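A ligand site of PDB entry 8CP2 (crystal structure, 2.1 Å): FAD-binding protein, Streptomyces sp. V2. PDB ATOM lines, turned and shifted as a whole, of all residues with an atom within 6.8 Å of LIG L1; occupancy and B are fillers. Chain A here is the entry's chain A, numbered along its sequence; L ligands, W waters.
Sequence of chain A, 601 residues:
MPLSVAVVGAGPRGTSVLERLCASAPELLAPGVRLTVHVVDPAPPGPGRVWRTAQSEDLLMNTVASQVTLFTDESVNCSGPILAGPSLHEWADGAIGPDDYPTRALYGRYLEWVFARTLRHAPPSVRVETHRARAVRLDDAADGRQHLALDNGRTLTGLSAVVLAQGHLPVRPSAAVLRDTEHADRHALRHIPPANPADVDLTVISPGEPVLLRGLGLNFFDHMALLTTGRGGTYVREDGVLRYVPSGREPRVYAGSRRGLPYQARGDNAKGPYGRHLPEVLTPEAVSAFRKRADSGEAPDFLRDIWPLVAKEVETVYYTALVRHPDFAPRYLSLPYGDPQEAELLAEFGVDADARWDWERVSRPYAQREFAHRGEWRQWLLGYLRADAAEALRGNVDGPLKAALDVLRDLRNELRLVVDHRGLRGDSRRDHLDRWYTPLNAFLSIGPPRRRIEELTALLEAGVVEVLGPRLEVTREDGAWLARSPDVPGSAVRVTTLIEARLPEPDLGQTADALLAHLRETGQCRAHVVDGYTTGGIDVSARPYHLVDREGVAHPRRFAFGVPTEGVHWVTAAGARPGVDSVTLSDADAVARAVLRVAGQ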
ATOM      1  N   ARG A  13      -8.365  -5.921  -2.876  1.00  0.00           N
ATOM      2  CA  ARG A  13      -8.889  -5.342  -1.592  1.00  0.00           C
ATOM      3  C   ARG A  13      -8.140  -5.963  -0.413  1.00  0.00           C
ATOM      4  O   ARG A  13      -7.704  -5.220   0.476  1.00  0.00           O
ATOM      5  CB  ARG A  13     -10.418  -5.445  -1.462  1.00  0.00           C
ATOM      6  CG  ARG A  13     -11.179  -4.280  -2.094  1.00  0.00           C
ATOM      7  CD  ARG A  13     -12.626  -4.182  -1.649  1.00  0.00           C
ATOM      8  NE  ARG A  13     -13.390  -3.141  -2.329  1.00  0.00           N
ATOM      9  CZ  ARG A  13     -14.065  -3.259  -3.489  1.00  0.00           C
ATOM     10  NH1 ARG A  13     -14.142  -4.402  -4.164  1.00  0.00           N
ATOM     11  NH2 ARG A  13     -14.722  -2.200  -3.947  1.00  0.00           N
ATOM     12  N   ARG A 276     -11.416  14.456 -13.159  1.00  0.00           N
ATOM     13  CA  ARG A 276     -12.761  13.994 -12.747  1.00  0.00           C
ATOM     14  C   ARG A 276     -13.648  15.214 -12.895  1.00  0.00           C
ATOM     15  O   ARG A 276     -13.272  16.268 -12.375  1.00  0.00           O
ATOM     16  CB  ARG A 276     -12.781  13.502 -11.304  1.00  0.00           C
ATOM     17  CG  ARG A 276     -14.002  12.678 -10.930  1.00  0.00           C
ATOM     18  CD  ARG A 276     -13.920  12.188  -9.488  1.00  0.00           C
ATOM     19  NE  ARG A 276     -14.198  13.235  -8.506  1.00  0.00           N
ATOM     20  CZ  ARG A 276     -15.400  13.535  -7.986  1.00  0.00           C
ATOM     21  NH1 ARG A 276     -16.472  12.913  -8.386  1.00  0.00           N
ATOM     22  NH2 ARG A 276     -15.509  14.487  -7.072  1.00  0.00           N
ATOM     23  N   ARG A 409     -19.837   8.159 -14.789  1.00  0.00           N
ATOM     24  CA  ARG A 409     -18.695   7.422 -14.168  1.00  0.00           C
ATOM     25  C   ARG A 409     -18.100   8.264 -13.010  1.00  0.00           C
ATOM     26  O   ARG A 409     -17.868   7.737 -11.929  1.00  0.00           O
ATOM     27  CB  ARG A 409     -17.642   7.056 -15.212  1.00  0.00           C
ATOM     28  CG  ARG A 409     -16.482   6.292 -14.605  1.00  0.00           C
ATOM     29  CD  ARG A 409     -15.199   6.614 -15.255  1.00  0.00           C
ATOM     30  NE  ARG A 409     -14.089   5.800 -14.781  1.00  0.00           N
ATOM     31  CZ  ARG A 409     -12.771   6.120 -14.903  1.00  0.00           C
ATOM     32  NH1 ARG A 409     -12.394   7.259 -15.495  1.00  0.00           N
ATOM     33  NH2 ARG A 409     -11.835   5.310 -14.378  1.00  0.00           N
ATOM     34  N   ARG A 412     -20.075   8.661  -9.451  1.00  0.00           N
ATOM     35  CA  ARG A 412     -20.312   7.483  -8.591  1.00  0.00           C
ATOM     36  C   ARG A 412     -19.966   7.780  -7.130  1.00  0.00           C
ATOM     37  O   ARG A 412     -20.708   7.306  -6.293  1.00  0.00           O
ATOM     38  CB  ARG A 412     -19.503   6.274  -9.008  1.00  0.00           C
ATOM     39  CG  ARG A 412     -20.090   5.538 -10.203  1.00  0.00           C
ATOM     40  CD  ARG A 412     -19.284   4.268 -10.153  1.00  0.00           C
ATOM     41  NE  ARG A 412     -19.241   3.951 -11.480  1.00  0.00           N
ATOM     42  CZ  ARG A 412     -18.191   3.717 -12.167  1.00  0.00           C
ATOM     43  NH1 ARG A 412     -17.000   3.582 -11.632  1.00  0.00           N
ATOM     44  NH2 ARG A 412     -18.438   3.480 -13.416  1.00  0.00           N
ATOM     45  N   ASN A 413     -18.916   8.552  -6.852  1.00  0.00           N
ATOM     46  CA  ASN A 413     -18.495   8.928  -5.469  1.00  0.00           C
ATOM     47  C   ASN A 413     -19.642   9.617  -4.718  1.00  0.00           C
ATOM     48  O   ASN A 413     -19.946   9.193  -3.602  1.00  0.00           O
ATOM     49  CB  ASN A 413     -17.234   9.793  -5.455  1.00  0.00           C
ATOM     50  CG  ASN A 413     -16.027   9.035  -5.973  1.00  0.00           C
ATOM     51  OD1 ASN A 413     -15.998   7.804  -5.896  1.00  0.00           O
ATOM     52  ND2 ASN A 413     -15.041   9.723  -6.534  1.00  0.00           N
ATOM     53  N   ARG A 416     -22.806   7.266  -4.285  1.00  0.00           N
ATOM     54  CA  ARG A 416     -22.551   6.341  -3.162  1.00  0.00           C
ATOM     55  C   ARG A 416     -22.892   7.068  -1.866  1.00  0.00           C
ATOM     56  O   ARG A 416     -23.611   6.480  -1.058  1.00  0.00           O
ATOM     57  CB  ARG A 416     -21.132   5.774  -3.177  1.00  0.00           C
ATOM     58  CG  ARG A 416     -20.871   4.830  -4.352  1.00  0.00           C
ATOM     59  CD  ARG A 416     -19.401   4.572  -4.414  1.00  0.00           C
ATOM     60  NE  ARG A 416     -19.138   3.672  -5.489  1.00  0.00           N
ATOM     61  CZ  ARG A 416     -18.132   3.769  -6.339  1.00  0.00           C
ATOM     62  NH1 ARG A 416     -17.285   4.782  -6.280  1.00  0.00           N
ATOM     63  NH2 ARG A 416     -17.983   2.871  -7.310  1.00  0.00           N
ATOM     64  N   VAL A 571     -22.092  -0.062  -6.520  1.00  0.00           N
ATOM     65  CA  VAL A 571     -21.029  -0.356  -7.522  1.00  0.00           C
ATOM     66  C   VAL A 571     -19.709  -0.628  -6.797  1.00  0.00           C
ATOM     67  O   VAL A 571     -18.799   0.205  -6.848  1.00  0.00           O
ATOM     68  CB  VAL A 571     -20.932   0.769  -8.580  1.00  0.00           C
ATOM     69  CG1 VAL A 571     -19.930   0.451  -9.673  1.00  0.00           C
ATOM     70  CG2 VAL A 571     -22.312   0.962  -9.197  1.00  0.00           C
ATOM     71  N   ALA A 573     -17.897  -3.186  -7.650  1.00  0.00           N
ATOM     72  CA  ALA A 573     -17.008  -3.860  -8.653  1.00  0.00           C
ATOM     73  C   ALA A 573     -16.214  -2.783  -9.430  1.00  0.00           C
ATOM     74  O   ALA A 573     -16.579  -2.452 -10.585  1.00  0.00           O
ATOM     75  CB  ALA A 573     -17.848  -4.741  -9.578  1.00  0.00           C
ATOM     76  N   ALA A 574     -15.231  -2.170  -8.788  1.00  0.00           N
ATOM     77  CA  ALA A 574     -14.434  -1.055  -9.327  1.00  0.00           C
ATOM     78  C   ALA A 574     -13.160  -0.944  -8.488  1.00  0.00           C
ATOM     79  O   ALA A 574     -13.280  -1.111  -7.256  1.00  0.00           O
ATOM     80  CB  ALA A 574     -15.217   0.227  -9.299  1.00  0.00           C
ATOM     81  N   GLY A 575     -12.013  -0.778  -9.136  1.00  0.00           N
ATOM     82  CA  GLY A 575     -10.728  -0.538  -8.467  1.00  0.00           C
ATOM     83  C   GLY A 575     -10.542   0.909  -8.064  1.00  0.00           C
ATOM     84  O   GLY A 575     -11.316   1.807  -8.483  1.00  0.00           O
ATOM     85  N   ALA A 576      -9.526   1.142  -7.250  1.00  0.00           N
ATOM     86  CA  ALA A 576      -9.064   2.483  -6.846  1.00  0.00           C
ATOM     87  C   ALA A 576      -8.585   3.337  -8.036  1.00  0.00           C
ATOM     88  O   ALA A 576      -7.883   2.836  -8.923  1.00  0.00           O
ATOM     89  CB  ALA A 576      -7.964   2.331  -5.860  1.00  0.00           C
ATOM     90  N   ARG A 577      -8.917   4.615  -8.000  1.00  0.00           N
ATOM     91  CA  ARG A 577      -8.380   5.663  -8.908  1.00  0.00           C
ATOM     92  C   ARG A 577      -7.509   6.587  -8.087  1.00  0.00           C
ATOM     93  O   ARG A 577      -7.847   6.943  -6.955  1.00  0.00           O
ATOM     94  CB  ARG A 577      -9.495   6.559  -9.463  1.00  0.00           C
ATOM     95  CG  ARG A 577     -10.259   5.957 -10.603  1.00  0.00           C
ATOM     96  CD  ARG A 577     -11.371   6.927 -10.962  1.00  0.00           C
ATOM     97  NE  ARG A 577     -10.878   8.080 -11.713  1.00  0.00           N
ATOM     98  CZ  ARG A 577     -11.665   9.009 -12.263  1.00  0.00           C
ATOM     99  NH1 ARG A 577     -12.999   8.911 -12.201  1.00  0.00           N
ATOM    100  NH2 ARG A 577     -11.090  10.029 -12.884  1.00  0.00           N
ATOM    101  N   PRO A 578      -6.409   7.059  -8.693  1.00  0.00           N
ATOM    102  CA  PRO A 578      -5.531   8.038  -8.054  1.00  0.00           C
ATOM    103  C   PRO A 578      -6.030   9.475  -8.190  1.00  0.00           C
ATOM    104  O   PRO A 578      -6.793   9.785  -9.145  1.00  0.00           O
ATOM    105  CB  PRO A 578      -4.222   7.870  -8.834  1.00  0.00           C
ATOM    106  CG  PRO A 578      -4.656   7.411 -10.218  1.00  0.00           C
ATOM    107  CD  PRO A 578      -5.959   6.660 -10.042  1.00  0.00           C
ATOM    108  N   VAL A 580      -8.195  11.279  -6.465  1.00  0.00           N
ATOM    109  CA  VAL A 580      -9.629  11.666  -6.293  1.00  0.00           C
ATOM    110  C   VAL A 580     -10.164  11.346  -4.876  1.00  0.00           C
ATOM    111  O   VAL A 580     -11.402  11.208  -4.724  1.00  0.00           O
ATOM    112  CB  VAL A 580     -10.502  11.011  -7.373  1.00  0.00           C
ATOM    113  CG1 VAL A 580     -10.089  11.464  -8.768  1.00  0.00           C
ATOM    114  CG2 VAL A 580     -10.483   9.502  -7.246  1.00  0.00           C
ATOM    115  N   ASP A 581      -9.306  11.248  -3.874  1.00  0.00           N
ATOM    116  CA  ASP A 581      -9.698  10.791  -2.515  1.00  0.00           C
ATOM    117  C   ASP A 581     -10.482   9.478  -2.599  1.00  0.00           C
ATOM    118  O   ASP A 581     -11.651   9.396  -2.187  1.00  0.00           O
ATOM    119  CB  ASP A 581     -10.456  11.897  -1.778  1.00  0.00           C
ATOM    120  CG  ASP A 581     -10.591  11.657  -0.274  1.00  0.00           C
ATOM    121  OD1 ASP A 581      -9.880  10.753   0.301  1.00  0.00           O
ATOM    122  OD2 ASP A 581     -11.383  12.408   0.323  1.00  0.00           O
ATOM    123  N   SER A 582      -9.853   8.472  -3.192  1.00  0.00           N
ATOM    124  CA  SER A 582     -10.470   7.131  -3.341  1.00  0.00           C
ATOM    125  C   SER A 582     -10.970   6.577  -1.984  1.00  0.00           C
ATOM    126  O   SER A 582     -10.189   6.399  -1.014  1.00  0.00           O
ATOM    127  CB  SER A 582      -9.514   6.176  -3.975  1.00  0.00           C
ATOM    128  OG  SER A 582     -10.068   4.871  -4.016  1.00  0.00           O
ATOM    129  N   VAL A 583     -12.268   6.272  -1.946  1.00  0.00           N
ATOM    130  CA  VAL A 583     -12.942   5.609  -0.811  1.00  0.00           C
ATOM    131  C   VAL A 583     -12.423   4.163  -0.698  1.00  0.00           C
ATOM    132  O   VAL A 583     -12.313   3.696   0.429  1.00  0.00           O
ATOM    133  CB  VAL A 583     -14.473   5.705  -0.927  1.00  0.00           C
ATOM    134  CG1 VAL A 583     -15.003   4.928  -2.123  1.00  0.00           C
ATOM    135  CG2 VAL A 583     -15.161   5.227   0.352  1.00  0.00           C
ATOM    136  N   THR A 584     -12.063   3.478  -1.799  1.00  0.00           N
ATOM    137  CA  THR A 584     -11.535   2.101  -1.741  1.00  0.00           C
ATOM    138  C   THR A 584     -10.244   2.057  -0.913  1.00  0.00           C
ATOM    139  O   THR A 584     -10.064   1.152  -0.103  1.00  0.00           O
ATOM    140  CB  THR A 584     -11.281   1.577  -3.156  1.00  0.00           C
ATOM    141  OG1 THR A 584     -12.477   1.893  -3.870  1.00  0.00           O
ATOM    142  CG2 THR A 584     -10.945   0.112  -3.169  1.00  0.00           C
ATOM    143  N   LEU A 585      -9.395   3.062  -1.068  1.00  0.00           N
ATOM    144  CA  LEU A 585      -8.102   3.206  -0.358  1.00  0.00           C
ATOM    145  C   LEU A 585      -8.336   3.686   1.076  1.00  0.00           C
ATOM    146  O   LEU A 585      -7.743   3.101   1.956  1.00  0.00           O
ATOM    147  CB  LEU A 585      -7.232   4.172  -1.153  1.00  0.00           C
ATOM    148  CG  LEU A 585      -6.868   3.680  -2.568  1.00  0.00           C
ATOM    149  CD1 LEU A 585      -6.066   4.726  -3.301  1.00  0.00           C
ATOM    150  CD2 LEU A 585      -6.074   2.404  -2.557  1.00  0.00           C
HETATM  151  N1  LIG L   1     -13.795   3.501  -6.972  1.00  0.00           N
HETATM  152  C1  LIG L   1     -14.216   4.718  -7.653  1.00  0.00           C
HETATM  153  C2  LIG L   1     -14.712   4.292  -9.047  1.00  0.00           C
HETATM  154  O1  LIG L   1     -14.111   4.315 -10.100  1.00  0.00           O
HETATM  155  C3  LIG L   1     -13.181   5.833  -7.593  1.00  0.00           C
HETATM  156  C4  LIG L   1     -12.534   5.818  -6.221  1.00  0.00           C
HETATM  157  O2  LIG L   1     -13.116   6.523  -5.332  1.00  0.00           O
HETATM  158  O3  LIG L   1     -11.559   4.945  -6.012  1.00  0.00           O
HETATM  159  O4  LIG L   1     -15.866   3.901  -9.031  1.00  0.00           O
HETATM  160  P1  LG2 L   2     -11.628  -9.964  -6.160  1.00  0.00           P
HETATM  161  O1  LG2 L   2     -10.632  -9.364  -7.111  1.00  0.00           O
HETATM  162  O2  LG2 L   2     -12.823 -10.779  -6.581  1.00  0.00           O
HETATM  163  O3  LG2 L   2     -10.736 -10.800  -5.169  1.00  0.00           O
HETATM  164  C1  LG2 L   2     -11.392 -11.636  -4.181  1.00  0.00           C
HETATM  165  C2  LG2 L   2     -10.463 -12.755  -3.821  1.00  0.00           C
HETATM  166  O4  LG2 L   2     -10.962 -13.418  -2.640  1.00  0.00           O
HETATM  167  C3  LG2 L   2     -10.287 -13.860  -4.882  1.00  0.00           C
HETATM  168  O5  LG2 L   2      -8.905 -14.089  -5.109  1.00  0.00           O
HETATM  169  C4  LG2 L   2     -10.868 -15.130  -4.248  1.00  0.00           C
HETATM  170  O6  LG2 L   2     -10.109 -16.278  -4.585  1.00  0.00           O
HETATM  171  C5  LG2 L   2     -10.715 -14.811  -2.755  1.00  0.00           C
HETATM  172  N1  LG2 L   2     -11.643 -15.541  -1.901  1.00  0.00           N
HETATM  173  C6  LG2 L   2     -13.033 -15.486  -1.918  1.00  0.00           C
HETATM  174  N2  LG2 L   2     -13.584 -16.285  -1.033  1.00  0.00           N
HETATM  175  C7  LG2 L   2     -12.491 -16.856  -0.385  1.00  0.00           C
HETATM  176  C8  LG2 L   2     -12.431 -17.779   0.670  1.00  0.00           C
HETATM  177  N3  LG2 L   2     -13.530 -18.294   1.213  1.00  0.00           N
HETATM  178  N4  LG2 L   2     -11.209 -18.115   1.138  1.00  0.00           N
HETATM  179  C9  LG2 L   2     -10.123 -17.578   0.541  1.00  0.00           C
HETATM  180  N5  LG2 L   2     -10.068 -16.725  -0.496  1.00  0.00           N
HETATM  181  C10 LG2 L   2     -11.296 -16.400  -0.902  1.00  0.00           C
HETATM  182  N6  LG2 L   2     -12.524  -3.024 -11.989  1.00  0.00           N
HETATM  183  C11 LG2 L   2     -11.882  -2.005 -12.540  1.00  0.00           C
HETATM  184  O7  LG2 L   2     -11.673  -0.986 -11.898  1.00  0.00           O
HETATM  185  N7  LG2 L   2     -11.479  -2.029 -13.858  1.00  0.00           N
HETATM  186  C12 LG2 L   2     -11.660  -3.130 -14.652  1.00  0.00           C
HETATM  187  O8  LG2 L   2     -11.240  -3.101 -15.794  1.00  0.00           O
HETATM  188  C13 LG2 L   2     -12.294  -4.258 -14.078  1.00  0.00           C
HETATM  189  N8  LG2 L   2     -12.471  -5.351 -14.789  1.00  0.00           N
HETATM  190  C14 LG2 L   2     -13.076  -6.422 -14.170  1.00  0.00           C
HETATM  191  C15 LG2 L   2     -13.249  -7.598 -14.910  1.00  0.00           C
HETATM  192  C16 LG2 L   2     -13.796  -8.726 -14.368  1.00  0.00           C
HETATM  193  C17 LG2 L   2     -13.933  -9.973 -15.213  1.00  0.00           C
HETATM  194  C18 LG2 L   2     -14.188  -8.712 -13.016  1.00  0.00           C
HETATM  195  C19 LG2 L   2     -14.819  -9.920 -12.412  1.00  0.00           C
HETATM  196  C20 LG2 L   2     -14.086  -7.549 -12.290  1.00  0.00           C
HETATM  197  C21 LG2 L   2     -13.503  -6.386 -12.821  1.00  0.00           C
HETATM  198  N9  LG2 L   2     -13.304  -5.209 -12.093  1.00  0.00           N
HETATM  199  C22 LG2 L   2     -12.687  -4.128 -12.688  1.00  0.00           C
HETATM  200  C23 LG2 L   2     -13.859  -5.025 -10.734  1.00  0.00           C
HETATM  201  C24 LG2 L   2     -13.190  -5.747  -9.578  1.00  0.00           C
HETATM  202  O9  LG2 L   2     -14.266  -5.851  -8.587  1.00  0.00           O
HETATM  203  C25 LG2 L   2     -12.064  -4.949  -8.937  1.00  0.00           C
HETATM  204  O10 LG2 L   2     -11.141  -4.461  -9.915  1.00  0.00           O
HETATM  205  C26 LG2 L   2     -11.327  -5.797  -7.892  1.00  0.00           C
HETATM  206  O11 LG2 L   2     -10.955  -7.028  -8.493  1.00  0.00           O
HETATM  207  C27 LG2 L   2     -12.152  -6.073  -6.647  1.00  0.00           C
HETATM  208  O12 LG2 L   2     -11.167  -6.578  -5.695  1.00  0.00           O
HETATM  209  P2  LG2 L   2     -11.591  -7.538  -4.486  1.00  0.00           P
HETATM  210  O13 LG2 L   2     -12.768  -6.937  -3.753  1.00  0.00           O
HETATM  211  O14 LG2 L   2     -10.327  -7.962  -3.819  1.00  0.00           O
HETATM  212  O15 LG2 L   2     -12.222  -8.840  -5.197  1.00  0.00           O
HETATM  213  O   HOH W   1     -15.242   6.899 -10.822  1.00  0.00           O
HETATM  214  O   HOH W   2     -14.534   1.019  -5.776  1.00  0.00           O
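The backbone NH of Gly 575 sits at hydrogen-bond distance from an oxygen (O7) of LG2 L2 (2.8 Å).
The backbone carbonyl oxygen (O) of Gly 575 is in hydrogen-bond range of a nitrogen (N1) of LIG L1 (3.4 Å).
OD1 of Asn 413 sits close to O2 of LIG L1, at 3.2 Å.
O3 of LIG L1 lies within hydrogen-bond range of OG of Ser 582 (2.5 Å).
The guanidinium group of Arg 416 is in salt-bridge range of an oxygen (O4) of LIG L1 (2.9 Å).
O14 of LG2 L2 lies within hydrogen-bond range of N of Arg 13, at 3.0 Å.
The guanidinium group (NH1) of Arg 412 lies within salt-bridge range of an oxygen (O4) of LIG L1 (2.9 Å).
An oxygen (O13) of LG2 L2 lies within salt-bridge range of the guanidinium group (NH1) of Arg 13.
N of Arg 577 is in hydrogen-bond range of O3 of LIG L1 (3.3 Å).
The side-chain hydroxyl (OG) of Ser 582 sits close to the backbone NH (N) of Thr 584, at 3.3 Å.
NH1 of Arg 416 lies within hydrogen-bond range of OD1 of Asn 413, at 3.3 Å.
The guanidinium group of Arg 416 lies within hydrogen-bond range of the backbone carbonyl oxygen of Val 571, 2.8 Å away.
N of Val 583 sits close to O2 of LIG L1 (3.5 Å).
Merely in contact with LIG L1: Ala 574 (3.7 Å), Ala 576 (3.6 Å) and Thr 584 (3.7 Å).
Ten residues have an atom within 4 Å of LIG L1: Arg 412, Asn 413, Arg 416, Ala 574, Gly 575, Ala 576, Arg 577, Ser 582, Val 583 and Thr 584.
The nearest printed residue that does not touch LIG L1 is Val 580 (4.3 Å).
Water W2 lies within hydrogen-bond range of N1 of LIG L1 (2.9 Å), O of Ala 574 (2.9 Å) and OG1 of Thr 584 (2.9 Å).
Water W1 lies within hydrogen-bond range of an oxygen (O1) of LIG L1 (2.9 Å), the backbone carbonyl oxygen (O) of Arg 409 (3.0 Å) and the guanidinium group (NH1) of Arg 577 (3.3 Å).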
